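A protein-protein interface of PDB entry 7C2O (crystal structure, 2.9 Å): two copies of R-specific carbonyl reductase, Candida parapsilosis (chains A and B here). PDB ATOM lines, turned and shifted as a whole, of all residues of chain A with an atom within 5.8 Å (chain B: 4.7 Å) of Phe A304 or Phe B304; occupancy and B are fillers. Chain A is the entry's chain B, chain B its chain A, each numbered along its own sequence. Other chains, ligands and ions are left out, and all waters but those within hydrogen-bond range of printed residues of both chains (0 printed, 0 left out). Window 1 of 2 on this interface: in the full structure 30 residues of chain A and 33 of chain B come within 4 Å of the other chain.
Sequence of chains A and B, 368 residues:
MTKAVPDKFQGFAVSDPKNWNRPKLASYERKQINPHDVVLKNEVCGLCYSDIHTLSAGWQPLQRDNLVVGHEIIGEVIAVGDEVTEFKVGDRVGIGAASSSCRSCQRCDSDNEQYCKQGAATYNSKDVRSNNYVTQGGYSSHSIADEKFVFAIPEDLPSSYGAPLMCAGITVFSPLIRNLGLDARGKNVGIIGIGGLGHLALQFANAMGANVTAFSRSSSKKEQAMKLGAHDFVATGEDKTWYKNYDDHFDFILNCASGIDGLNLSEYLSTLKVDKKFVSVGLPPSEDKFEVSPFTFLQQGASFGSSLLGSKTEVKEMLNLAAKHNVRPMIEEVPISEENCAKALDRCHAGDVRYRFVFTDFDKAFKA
Phe A290 touches its own counterpart, Phe B290. Phe A290 touches Phe B297, but with the chains exchanged Phe A297 does not touch Phe B290 (8.2 Å). Ser A303 touches Phe B304, and with the chains exchanged Phe A304 touches Ser B303. Ser A303 touches Gly B305, but with the chains exchanged Gly A305 does not touch Ser B303 (4.4 Å). Positions printed for both chains: 265, 278, 280, 290, 297, 302, 303, 304 and 305. Of the 17 pairs that touch across the chains among the printed residues, 9 have their exchanged pair printed and touching as well.
N of Phe B278 sits at hydrogen-bond distance from O of Ser B303, at 2.7 Å. O of Phe B278 is in hydrogen-bond range of N of Gly B305, at 2.9 Å. O of Ser A303 is in hydrogen-bond range of N of Phe A278 (2.6 Å). O of Phe A278 lies within hydrogen-bond range of N of Gly A305 (2.9 Å). The backbone NH (N) of Ser A280 sits at hydrogen-bond distance from the backbone carbonyl oxygen (O) of Gly A305. The backbone carbonyl oxygen (O) of Phe A297 sits at hydrogen-bond distance from the backbone NH (N) of Ala A302 (3.3 Å).
Among the printed residues, merely in contact across the chains: Ser A303 with Phe B304, Ala A302 with Gly B305, Phe A304 with Ser B303, Gly A305 with Ala B302, Val A292 with Phe B304, Phe A290 with Phe B297, Ser A303 with Gly B305, Phe A297 with Phe B304, Ser A306 with Phe B297, Phe A290 with Phe B290, Phe A304 with Phe B297, Pro A294 with Phe B290, Ser A303 with Ser B303, Ser A306 with Ala B302 and Pro A294 with Ser B280.
Phe A304 touches three residues of chain B. Phe B304 touches four residues of chain A. Of the printed residues of chain A, Ser B303 touches Ser A303 and Phe A304. Printed residues of chain B within 4 Å of Ser A303: Ser B303 (3.9 Å), Phe B304 (3.1 Å) and Gly B305 (3.6 Å). Of the printed residues of chain B, Pro A294 touches Ser B280 and Phe B290. Of the printed residues of chain B, Gly A305 touches Ala B302. Ser A280 touches none of the printed residues of chain B. The nearest printed residue of chain B that does not touch Ser A306 is Ser B303 (6.0 Å).
The backbone NH (N) of Val A292 lies within hydrogen-bond range of the backbone carbonyl oxygen (O) of Phe B290, at 2.6 Å. O of Phe B304 sits at hydrogen-bond distance from N of Phe A304.
Hydrophobic or aromatic side chains of chain B that line the printed part of chain A: Phe B290, Phe B297 and Phe B304. Of the 17 printed residues of chain A, 9 touch a printed residue of chain B.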
ATOM      1  N   ILE A 260       4.789  16.907  33.224  1.00  0.00           N
ATOM      2  CA  ILE A 260       3.887  16.482  32.160  1.00  0.00           C
ATOM      3  C   ILE A 260       3.833  14.957  32.163  1.00  0.00           C
ATOM      4  O   ILE A 260       3.640  14.314  31.125  1.00  0.00           O
ATOM      5  CB  ILE A 260       4.316  17.066  30.795  1.00  0.00           C
ATOM      6  CG1 ILE A 260       3.175  16.965  29.773  1.00  0.00           C
ATOM      7  CG2 ILE A 260       5.627  16.432  30.300  1.00  0.00           C
ATOM      8  CD1 ILE A 260       2.965  18.219  28.965  1.00  0.00           C
ATOM      9  N   LEU A 265      -4.641  17.019  32.312  1.00  0.00           N
ATOM     10  CA  LEU A 265      -5.064  18.106  31.440  1.00  0.00           C
ATOM     11  C   LEU A 265      -6.579  18.240  31.410  1.00  0.00           C
ATOM     12  O   LEU A 265      -7.097  19.343  31.211  1.00  0.00           O
ATOM     13  CB  LEU A 265      -4.520  17.886  30.030  1.00  0.00           C
ATOM     14  CG  LEU A 265      -4.374  19.155  29.188  1.00  0.00           C
ATOM     15  CD1 LEU A 265      -3.328  20.085  29.782  1.00  0.00           C
ATOM     16  CD2 LEU A 265      -4.040  18.814  27.742  1.00  0.00           C
ATOM     17  N   LYS A 277      -6.457  28.864  25.625  1.00  0.00           N
ATOM     18  CA  LYS A 277      -5.283  28.054  25.338  1.00  0.00           C
ATOM     19  C   LYS A 277      -4.607  27.603  26.626  1.00  0.00           C
ATOM     20  O   LYS A 277      -4.686  28.268  27.661  1.00  0.00           O
ATOM     21  CB  LYS A 277      -4.277  28.823  24.467  1.00  0.00           C
ATOM     22  CG  LYS A 277      -4.606  28.804  22.986  1.00  0.00           C
ATOM     23  CD  LYS A 277      -4.132  30.074  22.295  1.00  0.00           C
ATOM     24  CE  LYS A 277      -5.112  31.223  22.510  1.00  0.00           C
ATOM     25  NZ  LYS A 277      -6.453  30.959  21.905  1.00  0.00           N
ATOM     26  N   PHE A 278      -3.939  26.454  26.538  1.00  0.00           N
ATOM     27  CA  PHE A 278      -3.106  25.909  27.604  1.00  0.00           C
ATOM     28  C   PHE A 278      -1.682  25.844  27.065  1.00  0.00           C
ATOM     29  O   PHE A 278      -1.388  25.047  26.167  1.00  0.00           O
ATOM     30  CB  PHE A 278      -3.606  24.529  28.038  1.00  0.00           C
ATOM     31  CG  PHE A 278      -2.867  23.942  29.217  1.00  0.00           C
ATOM     32  CD1 PHE A 278      -3.394  24.028  30.495  1.00  0.00           C
ATOM     33  CD2 PHE A 278      -1.659  23.282  29.043  1.00  0.00           C
ATOM     34  CE1 PHE A 278      -2.727  23.481  31.578  1.00  0.00           C
ATOM     35  CE2 PHE A 278      -0.985  22.736  30.123  1.00  0.00           C
ATOM     36  CZ  PHE A 278      -1.522  22.836  31.391  1.00  0.00           C
ATOM     37  N   VAL A 279      -0.801  26.683  27.604  1.00  0.00           N
ATOM     38  CA  VAL A 279       0.572  26.808  27.126  1.00  0.00           C
ATOM     39  C   VAL A 279       1.512  26.229  28.174  1.00  0.00           C
ATOM     40  O   VAL A 279       1.378  26.525  29.369  1.00  0.00           O
ATOM     41  CB  VAL A 279       0.926  28.272  26.817  1.00  0.00           C
ATOM     42  CG1 VAL A 279       2.411  28.413  26.531  1.00  0.00           C
ATOM     43  CG2 VAL A 279       0.106  28.776  25.644  1.00  0.00           C
ATOM     44  N   SER A 280       2.459  25.410  27.729  1.00  0.00           N
ATOM     45  CA  SER A 280       3.478  24.832  28.592  1.00  0.00           C
ATOM     46  C   SER A 280       4.833  25.428  28.235  1.00  0.00           C
ATOM     47  O   SER A 280       5.192  25.499  27.055  1.00  0.00           O
ATOM     48  CB  SER A 280       3.513  23.309  28.448  1.00  0.00           C
ATOM     49  OG  SER A 280       2.585  22.691  29.321  1.00  0.00           O
ATOM     50  N   LEU A 283       9.418  22.955  29.447  1.00  0.00           N
ATOM     51  CA  LEU A 283       9.422  21.510  29.308  1.00  0.00           C
ATOM     52  C   LEU A 283      10.692  21.052  28.594  1.00  0.00           C
ATOM     53  O   LEU A 283      11.224  21.766  27.740  1.00  0.00           O
ATOM     54  CB  LEU A 283       8.195  21.046  28.530  1.00  0.00           C
ATOM     55  CG  LEU A 283       6.866  21.019  29.288  1.00  0.00           C
ATOM     56  CD1 LEU A 283       5.759  20.461  28.411  1.00  0.00           C
ATOM     57  CD2 LEU A 283       6.993  20.213  30.572  1.00  0.00           C
ATOM     58  N   PHE A 290       3.579  11.817  21.925  1.00  0.00           N
ATOM     59  CA  PHE A 290       2.469  11.459  22.794  1.00  0.00           C
ATOM     60  C   PHE A 290       1.166  11.497  22.004  1.00  0.00           C
ATOM     61  O   PHE A 290       1.086  12.090  20.925  1.00  0.00           O
ATOM     62  CB  PHE A 290       2.384  12.401  24.001  1.00  0.00           C
ATOM     63  CG  PHE A 290       2.426  13.860  23.638  1.00  0.00           C
ATOM     64  CD1 PHE A 290       3.630  14.543  23.591  1.00  0.00           C
ATOM     65  CD2 PHE A 290       1.261  14.551  23.348  1.00  0.00           C
ATOM     66  CE1 PHE A 290       3.672  15.884  23.259  1.00  0.00           C
ATOM     67  CE2 PHE A 290       1.298  15.893  23.014  1.00  0.00           C
ATOM     68  CZ  PHE A 290       2.505  16.559  22.970  1.00  0.00           C
ATOM     69  N   VAL A 292      -2.722  12.439  21.147  1.00  0.00           N
ATOM     70  CA  VAL A 292      -3.551  13.636  21.222  1.00  0.00           C
ATOM     71  C   VAL A 292      -4.921  13.313  20.642  1.00  0.00           C
ATOM     72  O   VAL A 292      -5.019  12.728  19.558  1.00  0.00           O
ATOM     73  CB  VAL A 292      -2.915  14.820  20.467  1.00  0.00           C
ATOM     74  CG1 VAL A 292      -3.825  16.025  20.510  1.00  0.00           C
ATOM     75  CG2 VAL A 292      -1.559  15.163  21.056  1.00  0.00           C
ATOM     76  N   SER A 293      -5.978  13.694  21.361  1.00  0.00           N
ATOM     77  CA  SER A 293      -7.340  13.477  20.901  1.00  0.00           C
ATOM     78  C   SER A 293      -8.103  14.794  20.866  1.00  0.00           C
ATOM     79  O   SER A 293      -7.971  15.616  21.781  1.00  0.00           O
ATOM     80  CB  SER A 293      -8.083  12.483  21.803  1.00  0.00           C
ATOM     81  OG  SER A 293      -9.449  12.398  21.438  1.00  0.00           O
ATOM     82  N   PRO A 294      -8.911  15.024  19.826  1.00  0.00           N
ATOM     83  CA  PRO A 294      -9.694  16.267  19.774  1.00  0.00           C
ATOM     84  C   PRO A 294     -10.808  16.328  20.804  1.00  0.00           C
ATOM     85  O   PRO A 294     -11.254  17.433  21.141  1.00  0.00           O
ATOM     86  CB  PRO A 294     -10.252  16.274  18.344  1.00  0.00           C
ATOM     87  CG  PRO A 294     -10.289  14.842  17.952  1.00  0.00           C
ATOM     88  CD  PRO A 294      -9.112  14.191  18.628  1.00  0.00           C
ATOM     89  N   PHE A 297     -10.360  18.672  23.974  1.00  0.00           N
ATOM     90  CA  PHE A 297     -10.572  20.111  23.896  1.00  0.00           C
ATOM     91  C   PHE A 297     -11.936  20.472  23.329  1.00  0.00           C
ATOM     92  O   PHE A 297     -12.184  21.651  23.051  1.00  0.00           O
ATOM     93  CB  PHE A 297      -9.477  20.766  23.050  1.00  0.00           C
ATOM     94  CG  PHE A 297      -8.100  20.232  23.319  1.00  0.00           C
ATOM     95  CD1 PHE A 297      -7.293  20.817  24.282  1.00  0.00           C
ATOM     96  CD2 PHE A 297      -7.607  19.151  22.605  1.00  0.00           C
ATOM     97  CE1 PHE A 297      -6.025  20.331  24.533  1.00  0.00           C
ATOM     98  CE2 PHE A 297      -6.343  18.661  22.853  1.00  0.00           C
ATOM     99  CZ  PHE A 297      -5.550  19.252  23.817  1.00  0.00           C
ATOM    100  N   ALA A 302     -10.923  24.644  23.639  1.00  0.00           N
ATOM    101  CA  ALA A 302      -9.609  24.994  24.152  1.00  0.00           C
ATOM    102  C   ALA A 302      -8.517  24.529  23.194  1.00  0.00           C
ATOM    103  O   ALA A 302      -8.775  23.911  22.158  1.00  0.00           O
ATOM    104  CB  ALA A 302      -9.408  24.394  25.542  1.00  0.00           C
ATOM    105  N   SER A 303      -7.271  24.838  23.548  1.00  0.00           N
ATOM    106  CA  SER A 303      -6.127  24.443  22.744  1.00  0.00           C
ATOM    107  C   SER A 303      -4.921  24.236  23.647  1.00  0.00           C
ATOM    108  O   SER A 303      -4.830  24.818  24.731  1.00  0.00           O
ATOM    109  CB  SER A 303      -5.816  25.478  21.656  1.00  0.00           C
ATOM    110  OG  SER A 303      -6.978  25.797  20.911  1.00  0.00           O
ATOM    111  N   PHE A 304      -4.002  23.390  23.188  1.00  0.00           N
ATOM    112  CA  PHE A 304      -2.779  23.062  23.906  1.00  0.00           C
ATOM    113  C   PHE A 304      -1.583  23.404  23.030  1.00  0.00           C
ATOM    114  O   PHE A 304      -1.605  23.166  21.819  1.00  0.00           O
ATOM    115  CB  PHE A 304      -2.757  21.578  24.294  1.00  0.00           C
ATOM    116  CG  PHE A 304      -1.434  21.100  24.820  1.00  0.00           C
ATOM    117  CD1 PHE A 304      -0.586  20.349  24.021  1.00  0.00           C
ATOM    118  CD2 PHE A 304      -1.044  21.389  26.119  1.00  0.00           C
ATOM    119  CE1 PHE A 304       0.633  19.903  24.505  1.00  0.00           C
ATOM    120  CE2 PHE A 304       0.175  20.943  26.610  1.00  0.00           C
ATOM    121  CZ  PHE A 304       1.013  20.200  25.802  1.00  0.00           C
ATOM    122  N   GLY A 305      -0.544  23.970  23.637  1.00  0.00           N
ATOM    123  CA  GLY A 305       0.617  24.378  22.872  1.00  0.00           C
ATOM    124  C   GLY A 305       1.801  24.655  23.772  1.00  0.00           C
ATOM    125  O   GLY A 305       1.729  24.526  24.995  1.00  0.00           O
ATOM    126  N   SER A 306       2.905  25.040  23.140  1.00  0.00           N
ATOM    127  CA  SER A 306       4.150  25.351  23.827  1.00  0.00           C
ATOM    128  C   SER A 306       4.534  26.806  23.574  1.00  0.00           C
ATOM    129  O   SER A 306       3.846  27.544  22.864  1.00  0.00           O
ATOM    130  CB  SER A 306       5.270  24.406  23.380  1.00  0.00           C
ATOM    131  OG  SER A 306       5.332  23.263  24.214  1.00  0.00           O
ATOM    132  N   LEU B 265      -0.066  14.871  12.119  1.00  0.00           N
ATOM    133  CA  LEU B 265      -0.239  16.148  12.801  1.00  0.00           C
ATOM    134  C   LEU B 265       1.077  16.913  12.884  1.00  0.00           C
ATOM    135  O   LEU B 265       1.094  18.142  12.755  1.00  0.00           O
ATOM    136  CB  LEU B 265      -0.824  15.916  14.193  1.00  0.00           C
ATOM    137  CG  LEU B 265      -1.139  17.158  15.022  1.00  0.00           C
ATOM    138  CD1 LEU B 265      -1.918  18.159  14.196  1.00  0.00           C
ATOM    139  CD2 LEU B 265      -1.914  16.776  16.269  1.00  0.00           C
ATOM    140  N   PHE B 278      -4.010  25.068  15.184  1.00  0.00           N
ATOM    141  CA  PHE B 278      -4.483  23.921  14.412  1.00  0.00           C
ATOM    142  C   PHE B 278      -5.766  23.453  15.092  1.00  0.00           C
ATOM    143  O   PHE B 278      -5.723  22.745  16.100  1.00  0.00           O
ATOM    144  CB  PHE B 278      -3.424  22.822  14.366  1.00  0.00           C
ATOM    145  CG  PHE B 278      -3.822  21.610  13.561  1.00  0.00           C
ATOM    146  CD1 PHE B 278      -3.311  21.412  12.291  1.00  0.00           C
ATOM    147  CD2 PHE B 278      -4.684  20.657  14.083  1.00  0.00           C
ATOM    148  CE1 PHE B 278      -3.664  20.297  11.551  1.00  0.00           C
ATOM    149  CE2 PHE B 278      -5.043  19.543  13.347  1.00  0.00           C
ATOM    150  CZ  PHE B 278      -4.530  19.363  12.079  1.00  0.00           C
ATOM    151  N   SER B 280      -9.231  21.326  15.081  1.00  0.00           N
ATOM    152  CA  SER B 280      -9.782  20.112  14.496  1.00  0.00           C
ATOM    153  C   SER B 280     -11.263  20.042  14.840  1.00  0.00           C
ATOM    154  O   SER B 280     -11.625  19.763  15.988  1.00  0.00           O
ATOM    155  CB  SER B 280      -9.041  18.877  15.004  1.00  0.00           C
ATOM    156  OG  SER B 280      -9.759  17.695  14.688  1.00  0.00           O
ATOM    157  N   PHE B 290      -4.223  11.295  17.314  1.00  0.00           N
ATOM    158  CA  PHE B 290      -3.076  11.815  16.584  1.00  0.00           C
ATOM    159  C   PHE B 290      -1.833  11.783  17.466  1.00  0.00           C
ATOM    160  O   PHE B 290      -1.915  11.860  18.696  1.00  0.00           O
ATOM    161  CB  PHE B 290      -3.334  13.246  16.105  1.00  0.00           C
ATOM    162  CG  PHE B 290      -4.658  13.433  15.421  1.00  0.00           C
ATOM    163  CD1 PHE B 290      -4.843  13.020  14.112  1.00  0.00           C
ATOM    164  CD2 PHE B 290      -5.717  14.034  16.084  1.00  0.00           C
ATOM    165  CE1 PHE B 290      -6.061  13.196  13.480  1.00  0.00           C
ATOM    166  CE2 PHE B 290      -6.936  14.212  15.458  1.00  0.00           C
ATOM    167  CZ  PHE B 290      -7.109  13.791  14.155  1.00  0.00           C
ATOM    168  N   PHE B 297       5.793  21.080  18.904  1.00  0.00           N
ATOM    169  CA  PHE B 297       5.037  22.191  19.466  1.00  0.00           C
ATOM    170  C   PHE B 297       5.928  23.388  19.770  1.00  0.00           C
ATOM    171  O   PHE B 297       5.467  24.538  19.710  1.00  0.00           O
ATOM    172  CB  PHE B 297       4.311  21.734  20.735  1.00  0.00           C
ATOM    173  CG  PHE B 297       2.999  21.053  20.479  1.00  0.00           C
ATOM    174  CD1 PHE B 297       2.056  21.647  19.658  1.00  0.00           C
ATOM    175  CD2 PHE B 297       2.698  19.833  21.064  1.00  0.00           C
ATOM    176  CE1 PHE B 297       0.843  21.040  19.419  1.00  0.00           C
ATOM    177  CE2 PHE B 297       1.481  19.219  20.826  1.00  0.00           C
ATOM    178  CZ  PHE B 297       0.554  19.824  20.001  1.00  0.00           C
ATOM    179  N   ALA B 302       2.962  26.534  18.029  1.00  0.00           N
ATOM    180  CA  ALA B 302       1.612  26.386  17.512  1.00  0.00           C
ATOM    181  C   ALA B 302       0.713  25.715  18.548  1.00  0.00           C
ATOM    182  O   ALA B 302       1.155  25.277  19.615  1.00  0.00           O
ATOM    183  CB  ALA B 302       1.632  25.597  16.205  1.00  0.00           C
ATOM    184  N   SER B 303      -0.575  25.631  18.226  1.00  0.00           N
ATOM    185  CA  SER B 303      -1.571  25.073  19.124  1.00  0.00           C
ATOM    186  C   SER B 303      -2.352  23.986  18.407  1.00  0.00           C
ATOM    187  O   SER B 303      -2.483  23.997  17.181  1.00  0.00           O
ATOM    188  CB  SER B 303      -2.553  26.147  19.627  1.00  0.00           C
ATOM    189  OG  SER B 303      -1.898  27.382  19.862  1.00  0.00           O
ATOM    190  N   PHE B 304      -2.870  23.045  19.191  1.00  0.00           N
ATOM    191  CA  PHE B 304      -3.848  22.076  18.721  1.00  0.00           C
ATOM    192  C   PHE B 304      -5.110  22.226  19.555  1.00  0.00           C
ATOM    193  O   PHE B 304      -5.042  22.258  20.788  1.00  0.00           O
ATOM    194  CB  PHE B 304      -3.322  20.643  18.817  1.00  0.00           C
ATOM    195  CG  PHE B 304      -4.350  19.608  18.464  1.00  0.00           C
ATOM    196  CD1 PHE B 304      -4.492  19.182  17.157  1.00  0.00           C
ATOM    197  CD2 PHE B 304      -5.182  19.072  19.433  1.00  0.00           C
ATOM    198  CE1 PHE B 304      -5.438  18.237  16.822  1.00  0.00           C
ATOM    199  CE2 PHE B 304      -6.132  18.132  19.104  1.00  0.00           C
ATOM    200  CZ  PHE B 304      -6.259  17.710  17.797  1.00  0.00           C
ATOM    201  N   GLY B 305      -6.258  22.302  18.887  1.00  0.00           N
ATOM    202  CA  GLY B 305      -7.512  22.478  19.586  1.00  0.00           C
ATOM    203  C   GLY B 305      -8.672  21.901  18.806  1.00  0.00           C
ATOM    204  O   GLY B 305      -8.503  21.303  17.741  1.00  0.00           O
